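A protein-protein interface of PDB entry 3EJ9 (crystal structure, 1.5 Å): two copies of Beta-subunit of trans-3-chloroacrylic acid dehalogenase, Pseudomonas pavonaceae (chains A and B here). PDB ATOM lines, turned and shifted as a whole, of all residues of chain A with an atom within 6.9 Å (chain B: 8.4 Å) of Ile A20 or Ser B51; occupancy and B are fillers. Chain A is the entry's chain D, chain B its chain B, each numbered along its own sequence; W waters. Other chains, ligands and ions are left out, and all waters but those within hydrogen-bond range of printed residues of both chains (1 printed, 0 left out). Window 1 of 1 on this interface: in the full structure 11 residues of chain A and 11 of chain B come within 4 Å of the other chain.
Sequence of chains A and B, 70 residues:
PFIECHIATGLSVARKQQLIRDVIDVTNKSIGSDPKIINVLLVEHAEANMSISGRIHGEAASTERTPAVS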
ATOM      1  N   PRO A   1      -1.802  21.510  19.821  1.00  0.00           N
ATOM      2  CA  PRO A   1      -2.132  22.491  18.797  1.00  0.00           C
ATOM      3  C   PRO A   1      -3.635  22.790  18.723  1.00  0.00           C
ATOM      4  O   PRO A   1      -4.450  22.022  19.225  1.00  0.00           O
ATOM      5  CB  PRO A   1      -1.661  21.808  17.511  1.00  0.00           C
ATOM      6  CG  PRO A   1      -0.525  20.930  17.938  1.00  0.00           C
ATOM      7  CD  PRO A   1      -0.711  20.606  19.400  1.00  0.00           C
ATOM      8  N   PHE A   2      -3.983  23.915  18.103  1.00  0.00           N
ATOM      9  CA  PHE A   2      -5.372  24.266  17.802  1.00  0.00           C
ATOM     10  C   PHE A   2      -5.461  24.522  16.305  1.00  0.00           C
ATOM     11  O   PHE A   2      -4.867  25.465  15.807  1.00  0.00           O
ATOM     12  CB  PHE A   2      -5.808  25.495  18.617  1.00  0.00           C
ATOM     13  CG  PHE A   2      -7.134  26.078  18.197  1.00  0.00           C
ATOM     14  CD1 PHE A   2      -8.247  25.261  18.032  1.00  0.00           C
ATOM     15  CD2 PHE A   2      -7.264  27.438  17.953  1.00  0.00           C
ATOM     16  CE1 PHE A   2      -9.482  25.790  17.637  1.00  0.00           C
ATOM     17  CE2 PHE A   2      -8.495  27.982  17.559  1.00  0.00           C
ATOM     18  CZ  PHE A   2      -9.605  27.152  17.399  1.00  0.00           C
ATOM     19  N   ARG A  15     -18.404  12.779   6.380  1.00  0.00           N
ATOM     20  CA  ARG A  15     -17.218  13.425   5.809  1.00  0.00           C
ATOM     21  C   ARG A  15     -16.553  14.400   6.772  1.00  0.00           C
ATOM     22  O   ARG A  15     -15.321  14.460   6.866  1.00  0.00           O
ATOM     23  CB  ARG A  15     -17.587  14.170   4.526  1.00  0.00           C
ATOM     24  CG  ARG A  15     -16.399  14.514   3.648  1.00  0.00           C
ATOM     25  CD  ARG A  15     -15.867  13.274   2.952  1.00  0.00           C
ATOM     26  NE  ARG A  15     -15.256  13.611   1.674  1.00  0.00           N
ATOM     27  CZ  ARG A  15     -15.912  13.640   0.517  1.00  0.00           C
ATOM     28  NH1 ARG A  15     -15.272  13.964  -0.598  1.00  0.00           N
ATOM     29  NH2 ARG A  15     -17.207  13.354   0.473  1.00  0.00           N
ATOM     30  N   LYS A  16     -17.368  15.175   7.481  1.00  0.00           N
ATOM     31  CA  LYS A  16     -16.830  16.139   8.439  1.00  0.00           C
ATOM     32  C   LYS A  16     -16.191  15.434   9.638  1.00  0.00           C
ATOM     33  O   LYS A  16     -15.124  15.839  10.100  1.00  0.00           O
ATOM     34  CB  LYS A  16     -17.905  17.137   8.871  1.00  0.00           C
ATOM     35  CG  LYS A  16     -18.299  18.120   7.768  1.00  0.00           C
ATOM     36  CD  LYS A  16     -19.307  19.157   8.235  1.00  0.00           C
ATOM     37  CE  LYS A  16     -20.731  18.668   8.087  1.00  0.00           C
ATOM     38  NZ  LYS A  16     -21.724  19.764   8.294  1.00  0.00           N
ATOM     39  N   GLN A  17     -16.827  14.360  10.109  1.00  0.00           N
ATOM     40  CA  GLN A  17     -16.289  13.563  11.210  1.00  0.00           C
ATOM     41  C   GLN A  17     -14.945  12.973  10.832  1.00  0.00           C
ATOM     42  O   GLN A  17     -13.990  13.039  11.610  1.00  0.00           O
ATOM     43  CB  GLN A  17     -17.242  12.424  11.579  1.00  0.00           C
ATOM     44  CG  GLN A  17     -18.342  12.795  12.542  1.00  0.00           C
ATOM     45  CD  GLN A  17     -19.046  11.571  13.109  1.00  0.00           C
ATOM     46  OE1 GLN A  17     -18.454  10.783  13.851  1.00  0.00           O
ATOM     47  NE2 GLN A  17     -20.321  11.411  12.767  1.00  0.00           N
ATOM     48  N   GLN A  18     -14.871  12.407   9.628  1.00  0.00           N
ATOM     49  CA  GLN A  18     -13.636  11.797   9.162  1.00  0.00           C
ATOM     50  C   GLN A  18     -12.534  12.828   8.967  1.00  0.00           C
ATOM     51  O   GLN A  18     -11.371  12.536   9.242  1.00  0.00           O
ATOM     52  CB  GLN A  18     -13.861  10.986   7.882  1.00  0.00           C
ATOM     53  CG  GLN A  18     -12.672  10.098   7.513  1.00  0.00           C
ATOM     54  CD  GLN A  18     -12.293   9.122   8.620  1.00  0.00           C
ATOM     55  OE1 GLN A  18     -13.139   8.384   9.131  1.00  0.00           O
ATOM     56  NE2 GLN A  18     -11.014   9.105   8.984  1.00  0.00           N
ATOM     57  N   LEU A  19     -12.898  14.024   8.506  1.00  0.00           N
ATOM     58  CA  LEU A  19     -11.929  15.114   8.371  1.00  0.00           C
ATOM     59  C   LEU A  19     -11.296  15.449   9.716  1.00  0.00           C
ATOM     60  O   LEU A  19     -10.081  15.597   9.808  1.00  0.00           O
ATOM     61  CB  LEU A  19     -12.574  16.357   7.742  1.00  0.00           C
ATOM     62  CG  LEU A  19     -11.711  17.618   7.551  1.00  0.00           C
ATOM     63  CD1 LEU A  19     -10.402  17.324   6.814  1.00  0.00           C
ATOM     64  CD2 LEU A  19     -12.506  18.683   6.823  1.00  0.00           C
ATOM     65  N   ILE A  20     -12.102  15.544  10.763  1.00  0.00           N
ATOM     66  CA  ILE A  20     -11.547  15.834  12.086  1.00  0.00           C
ATOM     67  C   ILE A  20     -10.603  14.722  12.540  1.00  0.00           C
ATOM     68  O   ILE A  20      -9.491  14.992  13.006  1.00  0.00           O
ATOM     69  CB  ILE A  20     -12.662  16.076  13.117  1.00  0.00           C
ATOM     70  CG1 ILE A  20     -13.441  17.332  12.731  1.00  0.00           C
ATOM     71  CG2 ILE A  20     -12.104  16.182  14.540  1.00  0.00           C
ATOM     72  CD1 ILE A  20     -14.641  17.599  13.590  1.00  0.00           C
ATOM     73  N   ARG A  21     -11.031  13.473  12.374  1.00  0.00           N
ATOM     74  CA  ARG A  21     -10.176  12.335  12.710  1.00  0.00           C
ATOM     75  C   ARG A  21      -8.850  12.400  11.951  1.00  0.00           C
ATOM     76  O   ARG A  21      -7.789  12.182  12.531  1.00  0.00           O
ATOM     77  CB  ARG A  21     -10.877  11.005  12.415  1.00  0.00           C
ATOM     78  CG  ARG A  21     -12.110  10.715  13.248  1.00  0.00           C
ATOM     79  CD  ARG A  21     -12.575   9.287  12.995  1.00  0.00           C
ATOM     80  NE  ARG A  21     -13.942   9.055  13.453  1.00  0.00           N
ATOM     81  CZ  ARG A  21     -14.284   8.753  14.703  1.00  0.00           C
ATOM     82  NH1 ARG A  21     -13.359   8.643  15.649  1.00  0.00           N
ATOM     83  NH2 ARG A  21     -15.561   8.561  15.009  1.00  0.00           N
ATOM     84  N   ASP A  22      -8.926  12.704  10.656  1.00  0.00           N
ATOM     85  CA  ASP A  22      -7.751  12.756   9.785  1.00  0.00           C
ATOM     86  C   ASP A  22      -6.814  13.902  10.142  1.00  0.00           C
ATOM     87  O   ASP A  22      -5.599  13.736  10.103  1.00  0.00           O
ATOM     88  CB  ASP A  22      -8.167  12.825   8.311  1.00  0.00           C
ATOM     89  CG  ASP A  22      -8.690  11.497   7.785  1.00  0.00           C
ATOM     90  OD1 ASP A  22      -9.198  11.475   6.647  1.00  0.00           O
ATOM     91  OD2 ASP A  22      -8.594  10.475   8.499  1.00  0.00           O
ATOM     92  N   VAL A  23      -7.378  15.051  10.512  1.00  0.00           N
ATOM     93  CA  VAL A  23      -6.585  16.185  10.985  1.00  0.00           C
ATOM     94  C   VAL A  23      -5.825  15.831  12.269  1.00  0.00           C
ATOM     95  O   VAL A  23      -4.628  16.121  12.386  1.00  0.00           O
ATOM     96  CB  VAL A  23      -7.451  17.455  11.174  1.00  0.00           C
ATOM     97  CG1 VAL A  23      -6.701  18.519  11.982  1.00  0.00           C
ATOM     98  CG2 VAL A  23      -7.865  18.021   9.817  1.00  0.00           C
ATOM     99  N   ILE A  24      -6.508  15.201  13.215  1.00  0.00           N
ATOM    100  CA  ILE A  24      -5.864  14.766  14.461  1.00  0.00           C
ATOM    101  C   ILE A  24      -4.721  13.800  14.145  1.00  0.00           C
ATOM    102  O   ILE A  24      -3.599  13.970  14.621  1.00  0.00           O
ATOM    103  CB  ILE A  24      -6.879  14.109  15.426  1.00  0.00           C
ATOM    104  CG1 ILE A  24      -7.928  15.138  15.868  1.00  0.00           C
ATOM    105  CG2 ILE A  24      -6.164  13.493  16.645  1.00  0.00           C
ATOM    106  CD1 ILE A  24      -9.178  14.543  16.493  1.00  0.00           C
ATOM    107  N   ASP A  25      -5.016  12.795  13.327  1.00  0.00           N
ATOM    108  CA  ASP A  25      -4.041  11.789  12.948  1.00  0.00           C
ATOM    109  C   ASP A  25      -2.794  12.371  12.286  1.00  0.00           C
ATOM    110  O   ASP A  25      -1.671  12.025  12.666  1.00  0.00           O
ATOM    111  CB  ASP A  25      -4.710  10.757  12.032  1.00  0.00           C
ATOM    112  CG  ASP A  25      -3.798   9.603  11.674  1.00  0.00           C
ATOM    113  OD1 ASP A  25      -3.701   9.272  10.470  1.00  0.00           O
ATOM    114  OD2 ASP A  25      -3.190   9.007  12.591  1.00  0.00           O
ATOM    115  N   PRO A  35      -2.623  13.235  20.819  1.00  0.00           N
ATOM    116  CA  PRO A  35      -3.999  13.675  20.602  1.00  0.00           C
ATOM    117  C   PRO A  35      -4.599  14.455  21.782  1.00  0.00           C
ATOM    118  O   PRO A  35      -5.452  15.312  21.564  1.00  0.00           O
ATOM    119  CB  PRO A  35      -4.750  12.360  20.368  1.00  0.00           C
ATOM    120  CG  PRO A  35      -3.732  11.486  19.734  1.00  0.00           C
ATOM    121  CD  PRO A  35      -2.436  11.824  20.423  1.00  0.00           C
ATOM    122  N   ILE A  38      -4.313  18.031  21.062  1.00  0.00           N
ATOM    123  CA  ILE A  38      -4.776  18.472  19.742  1.00  0.00           C
ATOM    124  C   ILE A  38      -6.252  18.872  19.814  1.00  0.00           C
ATOM    125  O   ILE A  38      -7.084  18.141  20.350  1.00  0.00           O
ATOM    126  CB  ILE A  38      -4.554  17.387  18.638  1.00  0.00           C
ATOM    127  CG1 ILE A  38      -3.072  16.988  18.550  1.00  0.00           C
ATOM    128  CG2 ILE A  38      -5.046  17.892  17.278  1.00  0.00           C
ATOM    129  CD1 ILE A  38      -2.784  15.816  17.617  1.00  0.00           C
ATOM    130  N   ASN A  39      -6.548  20.059  19.295  1.00  0.00           N
ATOM    131  CA  ASN A  39      -7.890  20.613  19.310  1.00  0.00           C
ATOM    132  C   ASN A  39      -8.240  21.058  17.908  1.00  0.00           C
ATOM    133  O   ASN A  39      -7.417  21.668  17.230  1.00  0.00           O
ATOM    134  CB  ASN A  39      -7.950  21.787  20.281  1.00  0.00           C
ATOM    135  CG  ASN A  39      -7.417  21.417  21.648  1.00  0.00           C
ATOM    136  OD1 ASN A  39      -8.120  20.812  22.460  1.00  0.00           O
ATOM    137  ND2 ASN A  39      -6.150  21.746  21.896  1.00  0.00           N
ATOM    138  N   VAL A  40      -9.453  20.736  17.472  1.00  0.00           N
ATOM    139  CA  VAL A  40      -9.857  21.001  16.093  1.00  0.00           C
ATOM    140  C   VAL A  40     -11.221  21.683  16.060  1.00  0.00           C
ATOM    141  O   VAL A  40     -12.146  21.273  16.756  1.00  0.00           O
ATOM    142  CB  VAL A  40      -9.893  19.698  15.234  1.00  0.00           C
ATOM    143  CG1 VAL A  40     -10.213  19.996  13.756  1.00  0.00           C
ATOM    144  CG2 VAL A  40      -8.572  18.956  15.325  1.00  0.00           C
ATOM    145  N   LEU A  41     -11.318  22.725  15.237  1.00  0.00           N
ATOM    146  CA  LEU A  41     -12.584  23.404  14.974  1.00  0.00           C
ATOM    147  C   LEU A  41     -12.812  23.440  13.472  1.00  0.00           C
ATOM    148  O   LEU A  41     -11.963  23.920  12.716  1.00  0.00           O
ATOM    149  CB  LEU A  41     -12.551  24.832  15.539  1.00  0.00           C
ATOM    150  CG  LEU A  41     -13.759  25.730  15.246  1.00  0.00           C
ATOM    151  CD1 LEU A  41     -15.029  25.198  15.877  1.00  0.00           C
ATOM    152  CD2 LEU A  41     -13.488  27.157  15.695  1.00  0.00           C
ATOM    153  N   LEU A  42     -13.958  22.919  13.051  1.00  0.00           N
ATOM    154  CA  LEU A  42     -14.344  22.957  11.656  1.00  0.00           C
ATOM    155  C   LEU A  42     -15.418  24.021  11.497  1.00  0.00           C
ATOM    156  O   LEU A  42     -16.415  24.011  12.219  1.00  0.00           O
ATOM    157  CB  LEU A  42     -14.884  21.589  11.250  1.00  0.00           C
ATOM    158  CG  LEU A  42     -15.179  21.368   9.771  1.00  0.00           C
ATOM    159  CD1 LEU A  42     -13.972  21.714   8.901  1.00  0.00           C
ATOM    160  CD2 LEU A  42     -15.615  19.924   9.546  1.00  0.00           C
ATOM    161  N   ALA B  46     -21.930  23.753  16.125  1.00  0.00           N
ATOM    162  CA  ALA B  46     -22.463  22.428  16.413  1.00  0.00           C
ATOM    163  C   ALA B  46     -21.385  21.623  17.140  1.00  0.00           C
ATOM    164  O   ALA B  46     -20.200  21.738  16.829  1.00  0.00           O
ATOM    165  CB  ALA B  46     -22.861  21.737  15.129  1.00  0.00           C
ATOM    166  N   GLU B  47     -21.801  20.808  18.104  1.00  0.00           N
ATOM    167  CA  GLU B  47     -20.869  19.988  18.887  1.00  0.00           C
ATOM    168  C   GLU B  47     -19.986  19.089  18.010  1.00  0.00           C
ATOM    169  O   GLU B  47     -18.805  18.885  18.307  1.00  0.00           O
ATOM    170  CB  GLU B  47     -21.641  19.142  19.913  1.00  0.00           C
ATOM    171  CG  GLU B  47     -22.293  19.957  21.034  1.00  0.00           C
ATOM    172  CD  GLU B  47     -21.393  20.170  22.246  1.00  0.00           C
ATOM    173  OE1 GLU B  47     -21.938  20.361  23.356  1.00  0.00           O
ATOM    174  OE2 GLU B  47     -20.153  20.153  22.103  1.00  0.00           O
ATOM    175  N   ALA B  48     -20.570  18.570  16.930  1.00  0.00           N
ATOM    176  CA  ALA B  48     -19.879  17.694  15.983  1.00  0.00           C
ATOM    177  C   ALA B  48     -18.699  18.375  15.293  1.00  0.00           C
ATOM    178  O   ALA B  48     -17.784  17.701  14.819  1.00  0.00           O
ATOM    179  CB  ALA B  48     -20.856  17.184  14.947  1.00  0.00           C
ATOM    180  N   ASN B  49     -18.724  19.705  15.239  1.00  0.00           N
ATOM    181  CA  ASN B  49     -17.683  20.468  14.547  1.00  0.00           C
ATOM    182  C   ASN B  49     -16.531  20.896  15.457  1.00  0.00           C
ATOM    183  O   ASN B  49     -15.648  21.637  15.023  1.00  0.00           O
ATOM    184  CB  ASN B  49     -18.290  21.695  13.851  1.00  0.00           C
ATOM    185  CG  ASN B  49     -19.186  21.328  12.663  1.00  0.00           C
ATOM    186  OD1 ASN B  49     -19.081  20.247  12.090  1.00  0.00           O
ATOM    187  ND2 ASN B  49     -20.070  22.245  12.294  1.00  0.00           N
ATOM    188  N   MET B  50     -16.552  20.422  16.703  1.00  0.00           N
ATOM    189  CA  MET B  50     -15.531  20.773  17.693  1.00  0.00           C
ATOM    190  C   MET B  50     -14.916  19.529  18.304  1.00  0.00           C
ATOM    191  O   MET B  50     -15.630  18.601  18.690  1.00  0.00           O
ATOM    192  CB  MET B  50     -16.130  21.625  18.814  1.00  0.00           C
ATOM    193  CG  MET B  50     -16.692  22.969  18.360  1.00  0.00           C
ATOM    194  SD  MET B  50     -17.219  23.993  19.741  1.00  0.00           S
ATOM    195  CE  MET B  50     -18.734  23.162  20.185  1.00  0.00           C
ATOM    196  N   SER B  51     -13.592  19.526  18.416  1.00  0.00           N
ATOM    197  CA  SER B  51     -12.874  18.444  19.085  1.00  0.00           C
ATOM    198  C   SER B  51     -11.826  19.006  20.038  1.00  0.00           C
ATOM    199  O   SER B  51     -10.918  19.725  19.627  1.00  0.00           O
ATOM    200  CB  SER B  51     -12.208  17.530  18.057  1.00  0.00           C
ATOM    201  OG  SER B  51     -11.366  16.586  18.699  1.00  0.00           O
ATOM    202  N   ILE B  52     -11.964  18.669  21.314  1.00  0.00           N
ATOM    203  CA  ILE B  52     -11.009  19.059  22.348  1.00  0.00           C
ATOM    204  C   ILE B  52     -10.262  17.817  22.772  1.00  0.00           C
ATOM    205  O   ILE B  52     -10.886  16.777  23.026  1.00  0.00           O
ATOM    206  CB  ILE B  52     -11.722  19.645  23.592  1.00  0.00           C
ATOM    207  CG1 ILE B  52     -12.603  20.838  23.215  1.00  0.00           C
ATOM    208  CG2 ILE B  52     -10.722  20.036  24.689  1.00  0.00           C
ATOM    209  CD1 ILE B  52     -11.853  22.132  22.916  1.00  0.00           C
ATOM    210  N   SER B  53      -8.938  17.925  22.859  1.00  0.00           N
ATOM    211  CA  SER B  53      -8.090  16.815  23.310  1.00  0.00           C
ATOM    212  C   SER B  53      -8.316  15.540  22.491  1.00  0.00           C
ATOM    213  O   SER B  53      -8.343  14.438  23.033  1.00  0.00           O
ATOM    214  CB  SER B  53      -8.281  16.550  24.811  1.00  0.00           C
ATOM    215  OG  SER B  53      -7.803  17.633  25.582  1.00  0.00           O
ATOM    216  N   GLY B  54      -8.470  15.714  21.180  1.00  0.00           N
ATOM    217  CA  GLY B  54      -8.620  14.602  20.239  1.00  0.00           C
ATOM    218  C   GLY B  54      -9.911  13.807  20.319  1.00  0.00           C
ATOM    219  O   GLY B  54     -10.040  12.772  19.658  1.00  0.00           O
ATOM    220  N   ARG B  55     -10.864  14.286  21.114  1.00  0.00           N
ATOM    221  CA  ARG B  55     -12.118  13.567  21.326  1.00  0.00           C
ATOM    222  C   ARG B  55     -13.114  13.832  20.203  1.00  0.00           C
ATOM    223  O   ARG B  55     -13.259  14.966  19.740  1.00  0.00           O
ATOM    224  CB  ARG B  55     -12.735  13.933  22.679  1.00  0.00           C
ATOM    225  CG  ARG B  55     -11.956  13.406  23.880  1.00  0.00           C
ATOM    226  CD  ARG B  55     -12.694  13.652  25.188  1.00  0.00           C
ATOM    227  NE  ARG B  55     -12.753  15.075  25.527  1.00  0.00           N
ATOM    228  CZ  ARG B  55     -11.891  15.704  26.323  1.00  0.00           C
ATOM    229  NH1 ARG B  55     -12.044  16.998  26.559  1.00  0.00           N
ATOM    230  NH2 ARG B  55     -10.883  15.049  26.884  1.00  0.00           N
ATOM    231  N   ILE B  56     -13.796  12.775  19.773  1.00  0.00           N
ATOM    232  CA  ILE B  56     -14.788  12.871  18.707  1.00  0.00           C
ATOM    233  C   ILE B  56     -16.184  12.817  19.323  1.00  0.00           C
ATOM    234  O   ILE B  56     -16.528  11.848  20.011  1.00  0.00           O
ATOM    235  CB  ILE B  56     -14.622  11.729  17.667  1.00  0.00           C
ATOM    236  CG1 ILE B  56     -13.203  11.717  17.068  1.00  0.00           C
ATOM    237  CG2 ILE B  56     -15.718  11.796  16.592  1.00  0.00           C
ATOM    238  CD1 ILE B  56     -12.808  12.965  16.285  1.00  0.00           C
ATOM    239  N   HIS B  57     -16.973  13.864  19.086  1.00  0.00           N
ATOM    240  CA  HIS B  57     -18.326  13.967  19.644  1.00  0.00           C
ATOM    241  C   HIS B  57     -19.181  12.761  19.257  1.00  0.00           C
ATOM    242  O   HIS B  57     -19.157  12.313  18.110  1.00  0.00           O
ATOM    243  CB  HIS B  57     -19.002  15.273  19.207  1.00  0.00           C
ATOM    244  CG  HIS B  57     -20.397  15.438  19.731  1.00  0.00           C
ATOM    245  ND1 HIS B  57     -20.666  15.784  21.037  1.00  0.00           N
ATOM    246  CD2 HIS B  57     -21.600  15.302  19.122  1.00  0.00           C
ATOM    247  CE1 HIS B  57     -21.975  15.853  21.212  1.00  0.00           C
ATOM    248  NE2 HIS B  57     -22.564  15.567  20.065  1.00  0.00           N
HETATM  249  O   HOH W   1     -21.623  19.864  11.184  1.00  0.00           O
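Water W1 lies within hydrogen-bond range of the side-chain amide oxygen of Asn B49 (2.7 Å) and the side-chain amino group of Lys A16 (2.9 Å).
No position is printed for both chains.
Of the 20 pairs that touch across the chains among the printed residues, none has its exchanged pair printed and touching as well.
The backbone NH of Leu A42 sits at hydrogen-bond distance from the backbone carbonyl oxygen of Asn B49, at 2.9 Å.
N of Val A40 lies within hydrogen-bond range of O of Ser B51 (2.8 Å).
The backbone NH (N) of Ser B53 lies within hydrogen-bond range of the backbone carbonyl oxygen (O) of Ile A38 (3.1 Å).
The backbone NH (N) of Ser B53 is in hydrogen-bond range of the side-chain amide oxygen (OD1) of Asn A39 (3.0 Å).
The backbone NH (N) of Gly B54 sits at hydrogen-bond distance from the backbone carbonyl oxygen (O) of Pro A35 (3.1 Å).
The backbone NH of Gly B54 sits at hydrogen-bond distance from the backbone carbonyl oxygen of Ile A38, at 2.9 Å.
O of Pro A35 lies close to O of Ser B53 (3.4 Å).
Of chain B, only Ala B48 (3.4 Å), Ser B51 (3.8 Å) and Ile B56 (3.7 Å) come within 4 Å of Ile A20.
Of the printed residues of chain B, Ile A24 touches Ser B51, Gly B54 and Ile B56.
Of the printed residues of chain B, Pro A35 touches Ser B53 and Gly B54.
Of the printed residues of chain A, Asn B49 touches Val A40, Leu A41 and Leu A42.
Of the printed residues of chain A, Ser B51 touches Ile A20, Ile A24, Asn A39 and Val A40.
Of the printed residues of chain A, Ile B56 touches Ile A20 (3.7 Å), Arg A21 (3.4 Å) and Ile A24 (3.96 Å).
The nearest residue of chain B that does not touch Ile A20 is Asn B49 (4.2 Å).
The nearest residue of chain A that does not touch Ser B51 is Ile A38 (4.2 Å).
The nearest printed residue of chain A that does not touch Ile B52 is Ile A38 (4.01 Å).
Among the printed residues, pairs that only touch across the chains: Ile A20 with Ala B48 (3.4 Å), Ile A20 with Ser B51 (3.8 Å), Ile A20 with Ile B56 (3.7 Å), Arg A21 with Ile B56 (3.4 Å), Ile A24 with Ser B51 (3.7 Å), Ile A24 with Gly B54 (3.7 Å), Ile A24 with Ile B56 (3.96 Å), Asn A39 with Ser B51 (3.2 Å), Asn A39 with Ile B52 (3.4 Å), Val A40 with Asn B49 (3.9 Å), Val A40 with Met B50 (3.5 Å), Leu A41 with Asn B49 (3.5 Å) and Leu A41 with Met B50 (3.7 Å).
Of the 12 printed residues of chain B, 8 touch a printed residue of chain A.
Printed residues of chain B that touch a printed residue of chain A: Ala B48, Asn B49, Met B50, Ser B51, Ile B52, Ser B53, Gly B54 and Ile B56.
Hydrophobic or aromatic side chains of chain B within 4 Å of the printed part of chain A: Met B50, Ile B52 and Ile B56.
Among the printed residues, 20 pairs touch across the chains.
Among the printed residues, no Asp or Glu carboxylate lies within 4 Å of a Lys or Arg side-chain nitrogen of the other chain.
The side-chain hydroxyl (OG) of Ser B51 sits at hydrogen-bond distance from the backbone carbonyl oxygen (O) of Arg B55 (2.7 Å).
The backbone carbonyl oxygen (O) of Pro A1 is in hydrogen-bond range of the backbone NH (N) of Asn A39.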
